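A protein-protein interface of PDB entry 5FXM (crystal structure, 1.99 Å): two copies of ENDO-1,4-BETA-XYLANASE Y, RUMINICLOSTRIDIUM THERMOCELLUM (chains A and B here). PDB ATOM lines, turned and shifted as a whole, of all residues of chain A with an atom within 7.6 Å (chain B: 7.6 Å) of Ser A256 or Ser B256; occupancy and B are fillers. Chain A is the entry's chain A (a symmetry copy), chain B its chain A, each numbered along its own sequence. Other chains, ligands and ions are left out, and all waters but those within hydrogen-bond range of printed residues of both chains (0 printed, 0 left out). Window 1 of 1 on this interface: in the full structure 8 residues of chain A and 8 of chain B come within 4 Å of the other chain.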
ATOM      1  N   TYR A  18       8.808   9.965   5.904  1.00  0.00           N
ATOM      2  CA  TYR A  18       9.170  10.847   6.980  1.00  0.00           C
ATOM      3  C   TYR A  18      10.137  10.137   7.937  1.00  0.00           C
ATOM      4  O   TYR A  18       9.889   8.997   8.356  1.00  0.00           O
ATOM      5  CB  TYR A  18       7.963  11.208   7.809  1.00  0.00           C
ATOM      6  CG  TYR A  18       6.990  12.241   7.305  1.00  0.00           C
ATOM      7  CD1 TYR A  18       7.371  13.583   7.061  1.00  0.00           C
ATOM      8  CD2 TYR A  18       5.638  11.917   7.194  1.00  0.00           C
ATOM      9  CE1 TYR A  18       6.425  14.544   6.691  1.00  0.00           C
ATOM     10  CE2 TYR A  18       4.693  12.879   6.842  1.00  0.00           C
ATOM     11  CZ  TYR A  18       5.086  14.170   6.587  1.00  0.00           C
ATOM     12  OH  TYR A  18       4.094  15.058   6.260  1.00  0.00           O
ATOM     13  N   ARG A 218      -2.014  20.393  14.210  1.00  0.00           N
ATOM     14  CA  ARG A 218      -1.893  19.712  12.920  1.00  0.00           C
ATOM     15  C   ARG A 218      -2.101  20.641  11.716  1.00  0.00           C
ATOM     16  O   ARG A 218      -2.196  20.189  10.571  1.00  0.00           O
ATOM     17  CB  ARG A 218      -2.914  18.545  12.856  1.00  0.00           C
ATOM     18  CG  ARG A 218      -2.892  17.590  14.047  1.00  0.00           C
ATOM     19  CD  ARG A 218      -1.517  16.944  14.225  1.00  0.00           C
ATOM     20  NE  ARG A 218      -1.146  16.304  12.965  1.00  0.00           N
ATOM     21  CZ  ARG A 218       0.074  16.203  12.439  1.00  0.00           C
ATOM     22  NH1 ARG A 218       1.168  16.634  13.051  1.00  0.00           N
ATOM     23  NH2 ARG A 218       0.190  15.605  11.272  1.00  0.00           N
ATOM     24  N   PHE A 221       3.258  24.163  10.554  1.00  0.00           N
ATOM     25  CA  PHE A 221       4.467  23.370  10.571  1.00  0.00           C
ATOM     26  C   PHE A 221       5.687  24.254  10.381  1.00  0.00           C
ATOM     27  O   PHE A 221       5.730  25.053   9.446  1.00  0.00           O
ATOM     28  CB  PHE A 221       4.443  22.309   9.478  1.00  0.00           C
ATOM     29  CG  PHE A 221       3.257  21.403   9.563  1.00  0.00           C
ATOM     30  CD1 PHE A 221       2.075  21.741   8.928  1.00  0.00           C
ATOM     31  CD2 PHE A 221       3.317  20.240  10.310  1.00  0.00           C
ATOM     32  CE1 PHE A 221       0.980  20.933   9.005  1.00  0.00           C
ATOM     33  CE2 PHE A 221       2.213  19.413  10.420  1.00  0.00           C
ATOM     34  CZ  PHE A 221       1.032  19.758   9.766  1.00  0.00           C
ATOM     35  N   ASP A 250       5.014  20.197  18.778  1.00  0.00           N
ATOM     36  CA  ASP A 250       5.505  18.851  19.094  1.00  0.00           C
ATOM     37  C   ASP A 250       6.749  18.667  18.229  1.00  0.00           C
ATOM     38  O   ASP A 250       6.635  18.671  17.013  1.00  0.00           O
ATOM     39  CB  ASP A 250       4.477  17.741  18.735  1.00  0.00           C
ATOM     40  CG  ASP A 250       3.254  17.716  19.653  1.00  0.00           C
ATOM     41  OD1 ASP A 250       3.293  18.317  20.741  1.00  0.00           O
ATOM     42  OD2 ASP A 250       2.241  17.088  19.285  1.00  0.00           O
ATOM     43  N   THR A 252       9.562  17.156  16.239  1.00  0.00           N
ATOM     44  CA  THR A 252       9.984  16.023  15.427  1.00  0.00           C
ATOM     45  C   THR A 252       9.889  16.496  13.970  1.00  0.00           C
ATOM     46  O   THR A 252       9.080  17.351  13.659  1.00  0.00           O
ATOM     47  CB  THR A 252       9.124  14.731  15.633  1.00  0.00           C
ATOM     48  OG1 THR A 252       9.402  13.796  14.602  1.00  0.00           O
ATOM     49  CG2 THR A 252       7.604  15.022  15.607  1.00  0.00           C
ATOM     50  N   SER A 253      10.732  15.947  13.101  1.00  0.00           N
ATOM     51  CA  SER A 253      10.586  16.165  11.681  1.00  0.00           C
ATOM     52  C   SER A 253       9.516  15.271  11.056  1.00  0.00           C
ATOM     53  O   SER A 253       9.221  15.443   9.885  1.00  0.00           O
ATOM     54  CB  SER A 253      11.917  15.989  10.932  1.00  0.00           C
ATOM     55  OG  SER A 253      12.564  14.771  11.208  1.00  0.00           O
ATOM     56  N   ASP A 254       8.939  14.320  11.806  1.00  0.00           N
ATOM     57  CA  ASP A 254       7.869  13.476  11.236  1.00  0.00           C
ATOM     58  C   ASP A 254       6.573  14.273  11.350  1.00  0.00           C
ATOM     59  O   ASP A 254       5.896  14.261  12.374  1.00  0.00           O
ATOM     60  CB  ASP A 254       7.807  12.124  11.918  1.00  0.00           C
ATOM     61  CG  ASP A 254       6.696  11.192  11.353  1.00  0.00           C
ATOM     62  OD1 ASP A 254       5.773  11.622  10.618  1.00  0.00           O
ATOM     63  OD2 ASP A 254       6.727  10.021  11.737  1.00  0.00           O
ATOM     64  N   PHE A 255       6.255  15.012  10.298  1.00  0.00           N
ATOM     65  CA  PHE A 255       5.078  15.880  10.319  1.00  0.00           C
ATOM     66  C   PHE A 255       3.743  15.132  10.242  1.00  0.00           C
ATOM     67  O   PHE A 255       2.668  15.749  10.342  1.00  0.00           O
ATOM     68  CB  PHE A 255       5.201  16.957   9.235  1.00  0.00           C
ATOM     69  CG  PHE A 255       6.278  17.999   9.510  1.00  0.00           C
ATOM     70  CD1 PHE A 255       6.844  18.180  10.777  1.00  0.00           C
ATOM     71  CD2 PHE A 255       6.692  18.831   8.499  1.00  0.00           C
ATOM     72  CE1 PHE A 255       7.822  19.137  10.981  1.00  0.00           C
ATOM     73  CE2 PHE A 255       7.673  19.798   8.702  1.00  0.00           C
ATOM     74  CZ  PHE A 255       8.225  19.966   9.946  1.00  0.00           C
ATOM     75  N   SER A 256       3.770  13.817  10.123  1.00  0.00           N
ATOM     76  CA  SER A 256       2.548  13.012  10.364  1.00  0.00           C
ATOM     77  C   SER A 256       2.267  12.867  11.868  1.00  0.00           C
ATOM     78  O   SER A 256       1.194  12.432  12.253  1.00  0.00           O
ATOM     79  CB  SER A 256       2.641  11.619   9.701  1.00  0.00           C
ATOM     80  OG  SER A 256       3.441  10.743  10.481  1.00  0.00           O
ATOM     81  N   LYS A 257       3.243  13.203  12.710  1.00  0.00           N
ATOM     82  CA  LYS A 257       3.097  13.095  14.169  1.00  0.00           C
ATOM     83  C   LYS A 257       3.245  14.446  14.892  1.00  0.00           C
ATOM     84  O   LYS A 257       2.605  14.667  15.885  1.00  0.00           O
ATOM     85  CB  LYS A 257       4.161  12.128  14.723  1.00  0.00           C
ATOM     86  CG  LYS A 257       4.080  10.715  14.169  1.00  0.00           C
ATOM     87  CD  LYS A 257       5.251   9.855  14.636  1.00  0.00           C
ATOM     88  CE  LYS A 257       5.201   8.470  14.005  1.00  0.00           C
ATOM     89  NZ  LYS A 257       3.948   7.789  14.402  1.00  0.00           N
ATOM     90  N   GLY A 258       4.092  15.341  14.392  1.00  0.00           N
ATOM     91  CA  GLY A 258       4.385  16.597  15.083  1.00  0.00           C
ATOM     92  C   GLY A 258       4.533  17.720  14.092  1.00  0.00           C
ATOM     93  O   GLY A 258       4.079  17.592  12.984  1.00  0.00           O
ATOM     94  N   ASN A 259       5.126  18.833  14.506  1.00  0.00           N
ATOM     95  CA  ASN A 259       5.064  20.015  13.685  1.00  0.00           C
ATOM     96  C   ASN A 259       6.244  21.005  13.762  1.00  0.00           C
ATOM     97  O   ASN A 259       6.130  22.116  13.304  1.00  0.00           O
ATOM     98  CB  ASN A 259       3.748  20.714  13.988  1.00  0.00           C
ATOM     99  CG  ASN A 259       3.703  21.344  15.361  1.00  0.00           C
ATOM    100  OD1 ASN A 259       4.560  21.117  16.244  1.00  0.00           O
ATOM    101  ND2 ASN A 259       2.640  22.116  15.585  1.00  0.00           N
ATOM    102  N   TYR A 285       9.705  17.552   2.891  1.00  0.00           N
ATOM    103  CA  TYR A 285       8.873  17.316   4.070  1.00  0.00           C
ATOM    104  C   TYR A 285       7.593  18.110   4.053  1.00  0.00           C
ATOM    105  O   TYR A 285       6.758  17.857   4.869  1.00  0.00           O
ATOM    106  CB  TYR A 285       9.674  17.614   5.389  1.00  0.00           C
ATOM    107  CG  TYR A 285      10.531  16.468   5.808  1.00  0.00           C
ATOM    108  CD1 TYR A 285      11.668  16.108   5.095  1.00  0.00           C
ATOM    109  CD2 TYR A 285      10.205  15.737   6.914  1.00  0.00           C
ATOM    110  CE1 TYR A 285      12.442  14.999   5.475  1.00  0.00           C
ATOM    111  CE2 TYR A 285      10.960  14.674   7.321  1.00  0.00           C
ATOM    112  CZ  TYR A 285      12.055  14.272   6.599  1.00  0.00           C
ATOM    113  OH  TYR A 285      12.721  13.154   7.075  1.00  0.00           O
ATOM    114  N   HIS A 288       2.384  17.392   2.789  1.00  0.00           N
ATOM    115  CA  HIS A 288       1.767  16.061   2.716  1.00  0.00           C
ATOM    116  C   HIS A 288       0.540  15.949   3.617  1.00  0.00           C
ATOM    117  O   HIS A 288      -0.271  15.041   3.437  1.00  0.00           O
ATOM    118  CB  HIS A 288       2.751  14.970   3.083  1.00  0.00           C
ATOM    119  CG  HIS A 288       4.031  15.071   2.339  1.00  0.00           C
ATOM    120  ND1 HIS A 288       4.088  14.923   0.984  1.00  0.00           N
ATOM    121  CD2 HIS A 288       5.290  15.373   2.746  1.00  0.00           C
ATOM    122  CE1 HIS A 288       5.340  15.049   0.574  1.00  0.00           C
ATOM    123  NE2 HIS A 288       6.085  15.357   1.625  1.00  0.00           N
ATOM    124  N   GLU A 289       0.411  16.850   4.589  1.00  0.00           N
ATOM    125  CA  GLU A 289      -0.655  16.702   5.565  1.00  0.00           C
ATOM    126  C   GLU A 289      -1.954  17.192   4.942  1.00  0.00           C
ATOM    127  O   GLU A 289      -2.027  18.299   4.418  1.00  0.00           O
ATOM    128  CB  GLU A 289      -0.315  17.378   6.895  1.00  0.00           C
ATOM    129  CG  GLU A 289       0.886  16.716   7.570  1.00  0.00           C
ATOM    130  CD  GLU A 289       0.840  15.162   7.593  1.00  0.00           C
ATOM    131  OE1 GLU A 289      -0.103  14.607   8.188  1.00  0.00           O
ATOM    132  OE2 GLU A 289       1.755  14.484   7.004  1.00  0.00           O
ATOM    133  N   HIS A 297       3.592   7.898   3.554  1.00  0.00           N
ATOM    134  CA  HIS A 297       4.832   8.519   3.960  1.00  0.00           C
ATOM    135  C   HIS A 297       5.240   8.133   5.395  1.00  0.00           C
ATOM    136  O   HIS A 297       6.271   8.544   5.931  1.00  0.00           O
ATOM    137  CB  HIS A 297       4.706  10.045   3.874  1.00  0.00           C
ATOM    138  CG  HIS A 297       4.475  10.569   2.496  1.00  0.00           C
ATOM    139  ND1 HIS A 297       5.227  10.169   1.409  1.00  0.00           N
ATOM    140  CD2 HIS A 297       3.576  11.465   2.026  1.00  0.00           C
ATOM    141  CE1 HIS A 297       4.792  10.793   0.331  1.00  0.00           C
ATOM    142  NE2 HIS A 297       3.825  11.609   0.689  1.00  0.00           N
ATOM    143  OXT HIS A 297       4.537   7.402   6.081  1.00  0.00           O
ATOM    144  N   TYR B  18      -7.594  13.590  22.267  1.00  0.00           N
ATOM    145  CA  TYR B  18      -6.822  12.384  22.399  1.00  0.00           C
ATOM    146  C   TYR B  18      -5.814  12.530  23.547  1.00  0.00           C
ATOM    147  O   TYR B  18      -5.093  13.536  23.631  1.00  0.00           O
ATOM    148  CB  TYR B  18      -6.000  12.132  21.160  1.00  0.00           C
ATOM    149  CG  TYR B  18      -6.655  11.564  19.929  1.00  0.00           C
ATOM    150  CD1 TYR B  18      -7.272  10.290  19.921  1.00  0.00           C
ATOM    151  CD2 TYR B  18      -6.546  12.243  18.716  1.00  0.00           C
ATOM    152  CE1 TYR B  18      -7.783   9.744  18.739  1.00  0.00           C
ATOM    153  CE2 TYR B  18      -7.039  11.692  17.535  1.00  0.00           C
ATOM    154  CZ  TYR B  18      -7.656  10.464  17.552  1.00  0.00           C
ATOM    155  OH  TYR B  18      -8.102   9.987  16.346  1.00  0.00           O
ATOM    156  N   ARG B 218      -1.234   4.435   9.205  1.00  0.00           N
ATOM    157  CA  ARG B 218      -2.311   5.389   9.477  1.00  0.00           C
ATOM    158  C   ARG B 218      -3.688   4.912   8.992  1.00  0.00           C
ATOM    159  O   ARG B 218      -4.662   5.669   8.997  1.00  0.00           O
ATOM    160  CB  ARG B 218      -1.973   6.750   8.814  1.00  0.00           C
ATOM    161  CG  ARG B 218      -0.584   7.303   9.126  1.00  0.00           C
ATOM    162  CD  ARG B 218      -0.381   7.499  10.630  1.00  0.00           C
ATOM    163  NE  ARG B 218      -1.463   8.342  11.132  1.00  0.00           N
ATOM    164  CZ  ARG B 218      -2.062   8.265  12.318  1.00  0.00           C
ATOM    165  NH1 ARG B 218      -1.693   7.416  13.267  1.00  0.00           N
ATOM    166  NH2 ARG B 218      -3.042   9.110  12.566  1.00  0.00           N
ATOM    167  N   PHE B 221      -6.235   0.587  13.150  1.00  0.00           N
ATOM    168  CA  PHE B 221      -6.134   1.006  14.530  1.00  0.00           C
ATOM    169  C   PHE B 221      -6.663  -0.074  15.456  1.00  0.00           C
ATOM    170  O   PHE B 221      -7.772  -0.569  15.255  1.00  0.00           O
ATOM    171  CB  PHE B 221      -6.909   2.295  14.772  1.00  0.00           C
ATOM    172  CG  PHE B 221      -6.477   3.417  13.882  1.00  0.00           C
ATOM    173  CD1 PHE B 221      -7.059   3.583  12.637  1.00  0.00           C
ATOM    174  CD2 PHE B 221      -5.466   4.274  14.277  1.00  0.00           C
ATOM    175  CE1 PHE B 221      -6.671   4.592  11.808  1.00  0.00           C
ATOM    176  CE2 PHE B 221      -5.039   5.295  13.445  1.00  0.00           C
ATOM    177  CZ  PHE B 221      -5.641   5.458  12.199  1.00  0.00           C
ATOM    178  N   ASP B 250       2.519   1.555  16.127  1.00  0.00           N
ATOM    179  CA  ASP B 250       3.121   2.588  16.976  1.00  0.00           C
ATOM    180  C   ASP B 250       2.216   2.676  18.201  1.00  0.00           C
ATOM    181  O   ASP B 250       1.057   3.035  18.060  1.00  0.00           O
ATOM    182  CB  ASP B 250       3.162   3.980  16.283  1.00  0.00           C
ATOM    183  CG  ASP B 250       4.172   4.066  15.137  1.00  0.00           C
ATOM    184  OD1 ASP B 250       5.059   3.201  15.036  1.00  0.00           O
ATOM    185  OD2 ASP B 250       4.079   5.009  14.326  1.00  0.00           O
ATOM    186  N   THR B 252       0.416   3.897  21.271  1.00  0.00           N
ATOM    187  CA  THR B 252      -0.113   5.062  21.968  1.00  0.00           C
ATOM    188  C   THR B 252      -1.627   5.048  21.711  1.00  0.00           C
ATOM    189  O   THR B 252      -2.067   4.549  20.691  1.00  0.00           O
ATOM    190  CB  THR B 252       0.501   6.423  21.500  1.00  0.00           C
ATOM    191  OG1 THR B 252      -0.277   7.501  21.999  1.00  0.00           O
ATOM    192  CG2 THR B 252       0.550   6.553  19.958  1.00  0.00           C
ATOM    193  N   SER B 253      -2.404   5.577  22.651  1.00  0.00           N
ATOM    194  CA  SER B 253      -3.810   5.803  22.416  1.00  0.00           C
ATOM    195  C   SER B 253      -4.076   7.078  21.617  1.00  0.00           C
ATOM    196  O   SER B 253      -5.217   7.315  21.258  1.00  0.00           O
ATOM    197  CB  SER B 253      -4.615   5.828  23.725  1.00  0.00           C
ATOM    198  OG  SER B 253      -4.100   6.715  24.688  1.00  0.00           O
ATOM    199  N   ASP B 254      -3.054   7.902  21.342  1.00  0.00           N
ATOM    200  CA  ASP B 254      -3.280   9.115  20.531  1.00  0.00           C
ATOM    201  C   ASP B 254      -3.249   8.680  19.069  1.00  0.00           C
ATOM    202  O   ASP B 254      -2.195   8.584  18.447  1.00  0.00           O
ATOM    203  CB  ASP B 254      -2.271  10.197  20.859  1.00  0.00           C
ATOM    204  CG  ASP B 254      -2.465  11.501  20.033  1.00  0.00           C
ATOM    205  OD1 ASP B 254      -3.191  11.542  19.010  1.00  0.00           O
ATOM    206  OD2 ASP B 254      -1.797  12.474  20.393  1.00  0.00           O
ATOM    207  N   PHE B 255      -4.419   8.365  18.535  1.00  0.00           N
ATOM    208  CA  PHE B 255      -4.508   7.858  17.166  1.00  0.00           C
ATOM    209  C   PHE B 255      -4.258   8.916  16.086  1.00  0.00           C
ATOM    210  O   PHE B 255      -4.216   8.593  14.886  1.00  0.00           O
ATOM    211  CB  PHE B 255      -5.839   7.126  16.962  1.00  0.00           C
ATOM    212  CG  PHE B 255      -5.949   5.807  17.719  1.00  0.00           C
ATOM    213  CD1 PHE B 255      -4.832   5.146  18.244  1.00  0.00           C
ATOM    214  CD2 PHE B 255      -7.175   5.208  17.864  1.00  0.00           C
ATOM    215  CE1 PHE B 255      -4.978   3.953  18.926  1.00  0.00           C
ATOM    216  CE2 PHE B 255      -7.324   4.004  18.546  1.00  0.00           C
ATOM    217  CZ  PHE B 255      -6.226   3.364  19.061  1.00  0.00           C
ATOM    218  N   SER B 256      -4.036  10.160  16.469  1.00  0.00           N
ATOM    219  CA  SER B 256      -3.478  11.154  15.522  1.00  0.00           C
ATOM    220  C   SER B 256      -1.968  10.948  15.328  1.00  0.00           C
ATOM    221  O   SER B 256      -1.380  11.522  14.426  1.00  0.00           O
ATOM    222  CB  SER B 256      -3.766  12.603  15.977  1.00  0.00           C
ATOM    223  OG  SER B 256      -2.869  12.995  17.005  1.00  0.00           O
ATOM    224  N   LYS B 257      -1.340  10.155  16.195  1.00  0.00           N
ATOM    225  CA  LYS B 257       0.104   9.892  16.120  1.00  0.00           C
ATOM    226  C   LYS B 257       0.437   8.404  15.909  1.00  0.00           C
ATOM    227  O   LYS B 257       1.398   8.092  15.257  1.00  0.00           O
ATOM    228  CB  LYS B 257       0.782  10.362  17.421  1.00  0.00           C
ATOM    229  CG  LYS B 257       0.621  11.845  17.717  1.00  0.00           C
ATOM    230  CD  LYS B 257       1.177  12.212  19.091  1.00  0.00           C
ATOM    231  CE  LYS B 257       0.932  13.681  19.407  1.00  0.00           C
ATOM    232  NZ  LYS B 257       1.611  14.525  18.399  1.00  0.00           N
ATOM    233  N   GLY B 258      -0.357   7.494  16.465  1.00  0.00           N
ATOM    234  CA  GLY B 258      -0.045   6.065  16.419  1.00  0.00           C
ATOM    235  C   GLY B 258      -1.300   5.259  16.230  1.00  0.00           C
ATOM    236  O   GLY B 258      -2.288   5.798  15.801  1.00  0.00           O
ATOM    237  N   ASN B 259      -1.247   3.961  16.504  1.00  0.00           N
ATOM    238  CA  ASN B 259      -2.335   3.107  16.100  1.00  0.00           C
ATOM    239  C   ASN B 259      -2.631   1.865  16.965  1.00  0.00           C
ATOM    240  O   ASN B 259      -3.346   0.990  16.540  1.00  0.00           O
ATOM    241  CB  ASN B 259      -2.095   2.715  14.651  1.00  0.00           C
ATOM    242  CG  ASN B 259      -0.932   1.767  14.468  1.00  0.00           C
ATOM    243  OD1 ASN B 259      -0.109   1.514  15.376  1.00  0.00           O
ATOM    244  ND2 ASN B 259      -0.812   1.263  13.240  1.00  0.00           N
ATOM    245  N   TYR B 285     -12.531   7.155  20.974  1.00  0.00           N
ATOM    246  CA  TYR B 285     -11.256   7.265  20.268  1.00  0.00           C
ATOM    247  C   TYR B 285     -11.351   6.864  18.820  1.00  0.00           C
ATOM    248  O   TYR B 285     -10.421   7.089  18.106  1.00  0.00           O
ATOM    249  CB  TYR B 285     -10.143   6.421  20.988  1.00  0.00           C
ATOM    250  CG  TYR B 285      -9.529   7.147  22.137  1.00  0.00           C
ATOM    251  CD1 TYR B 285     -10.233   7.383  23.312  1.00  0.00           C
ATOM    252  CD2 TYR B 285      -8.245   7.605  22.051  1.00  0.00           C
ATOM    253  CE1 TYR B 285      -9.658   8.108  24.369  1.00  0.00           C
ATOM    254  CE2 TYR B 285      -7.655   8.284  23.079  1.00  0.00           C
ATOM    255  CZ  TYR B 285      -8.352   8.572  24.223  1.00  0.00           C
ATOM    256  OH  TYR B 285      -7.672   9.306  25.182  1.00  0.00           O
ATOM    257  N   HIS B 288     -11.872   9.216  13.978  1.00  0.00           N
ATOM    258  CA  HIS B 288     -11.539  10.629  13.748  1.00  0.00           C
ATOM    259  C   HIS B 288     -10.524  10.801  12.622  1.00  0.00           C
ATOM    260  O   HIS B 288     -10.384  11.900  12.086  1.00  0.00           O
ATOM    261  CB  HIS B 288     -11.001  11.285  15.002  1.00  0.00           C
ATOM    262  CG  HIS B 288     -11.868  11.066  16.187  1.00  0.00           C
ATOM    263  ND1 HIS B 288     -13.138  11.561  16.249  1.00  0.00           N
ATOM    264  CD2 HIS B 288     -11.678  10.351  17.324  1.00  0.00           C
ATOM    265  CE1 HIS B 288     -13.687  11.234  17.409  1.00  0.00           C
ATOM    266  NE2 HIS B 288     -12.829  10.469  18.066  1.00  0.00           N
ATOM    267  N   GLU B 289      -9.809   9.732  12.274  1.00  0.00           N
ATOM    268  CA  GLU B 289      -8.728   9.876  11.314  1.00  0.00           C
ATOM    269  C   GLU B 289      -9.326   9.928   9.915  1.00  0.00           C
ATOM    270  O   GLU B 289     -10.108   9.065   9.529  1.00  0.00           O
ATOM    271  CB  GLU B 289      -7.657   8.798  11.487  1.00  0.00           C
ATOM    272  CG  GLU B 289      -6.955   8.916  12.840  1.00  0.00           C
ATOM    273  CD  GLU B 289      -6.529  10.362  13.223  1.00  0.00           C
ATOM    274  OE1 GLU B 289      -5.721  10.956  12.483  1.00  0.00           O
ATOM    275  OE2 GLU B 289      -7.009  10.916  14.274  1.00  0.00           O
ATOM    276  N   HIS B 297      -8.811  17.492  17.763  1.00  0.00           N
ATOM    277  CA  HIS B 297      -8.702  16.486  18.794  1.00  0.00           C
ATOM    278  C   HIS B 297      -7.263  16.345  19.327  1.00  0.00           C
ATOM    279  O   HIS B 297      -6.954  15.551  20.218  1.00  0.00           O
ATOM    280  CB  HIS B 297      -9.164  15.128  18.252  1.00  0.00           C
ATOM    281  CG  HIS B 297     -10.602  15.080  17.853  1.00  0.00           C
ATOM    282  ND1 HIS B 297     -11.617  15.555  18.658  1.00  0.00           N
ATOM    283  CD2 HIS B 297     -11.197  14.611  16.731  1.00  0.00           C
ATOM    284  CE1 HIS B 297     -12.771  15.385  18.043  1.00  0.00           C
ATOM    285  NE2 HIS B 297     -12.543  14.779  16.898  1.00  0.00           N
ATOM    286  OXT HIS B 297      -6.346  17.015  18.868  1.00  0.00           O
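Of the 16 printed residues of chain A, 3 touch a printed residue of chain B. Printed residues of chain A that touch a printed residue of chain B: Asp A250, Ser A256 and Lys A257. Of the 16 printed residues of chain B, 3 touch a printed residue of chain A.
Asp A250 touches Lys B257, and with the chains exchanged Lys A257 touches Asp B250. Ser B256 touches its own counterpart, Ser A256. Lys B257 touches its own counterpart, Lys A257. 16 positions are printed for both chains.
The backbone carbonyl oxygen (O) of Ser A256 lies close to the backbone carbonyl oxygen (O) of Ser B256. O of Lys B257 sits at hydrogen-bond distance from NZ of Lys A257 (2.7 Å). The side-chain amino group (NZ) of Lys B257 is in salt-bridge range of the side-chain carboxylate (OD2) of Asp A250 (2.8 Å). The side-chain amino group (NZ) of Lys A257 is in salt-bridge range of the side-chain carboxylate (OD2) of Asp B250 (2.8 Å).
NH2 of Arg B218 is in hydrogen-bond range of O of Ser B256 (3.5 Å). The side-chain amide oxygen (OD1) of Asn A259 sits at hydrogen-bond distance from the backbone NH (N) of Asp A250 (2.7 Å). NH2 of Arg A218 is in hydrogen-bond range of O of Ser A256, at 3.5 Å. The side-chain hydroxyl (OG) of Ser B256 lies within hydrogen-bond range of the side-chain carboxylate (OD1) of Asp B254, 2.5 Å away. The side-chain hydroxyl (OG) of Ser A256 sits at hydrogen-bond distance from the side-chain carboxylate (OD1) of Asp A254, at 2.5 Å. N of Asp B250 lies within hydrogen-bond range of OD1 of Asn B259, 2.7 Å away.
Ser A256 touches one residue of chain B. Of the printed residues of chain B, Asp A250 touches Lys B257 (2.8 Å). Of the printed residues of chain A, Asp B250 touches Lys A257. Printed residues of chain B within 4 Å of Lys A257: Asp B250 (2.8 Å) and Lys B257 (2.7 Å). Phe A221 touches none of the printed residues of chain B. Arg B218 touches none of the printed residues of chain A. The nearest printed residue of chain A that does not touch Ser B256 is Lys A257 (4.8 Å). The nearest printed residue of chain B that does not touch Asp A250 is Asp B254 (6.2 Å).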
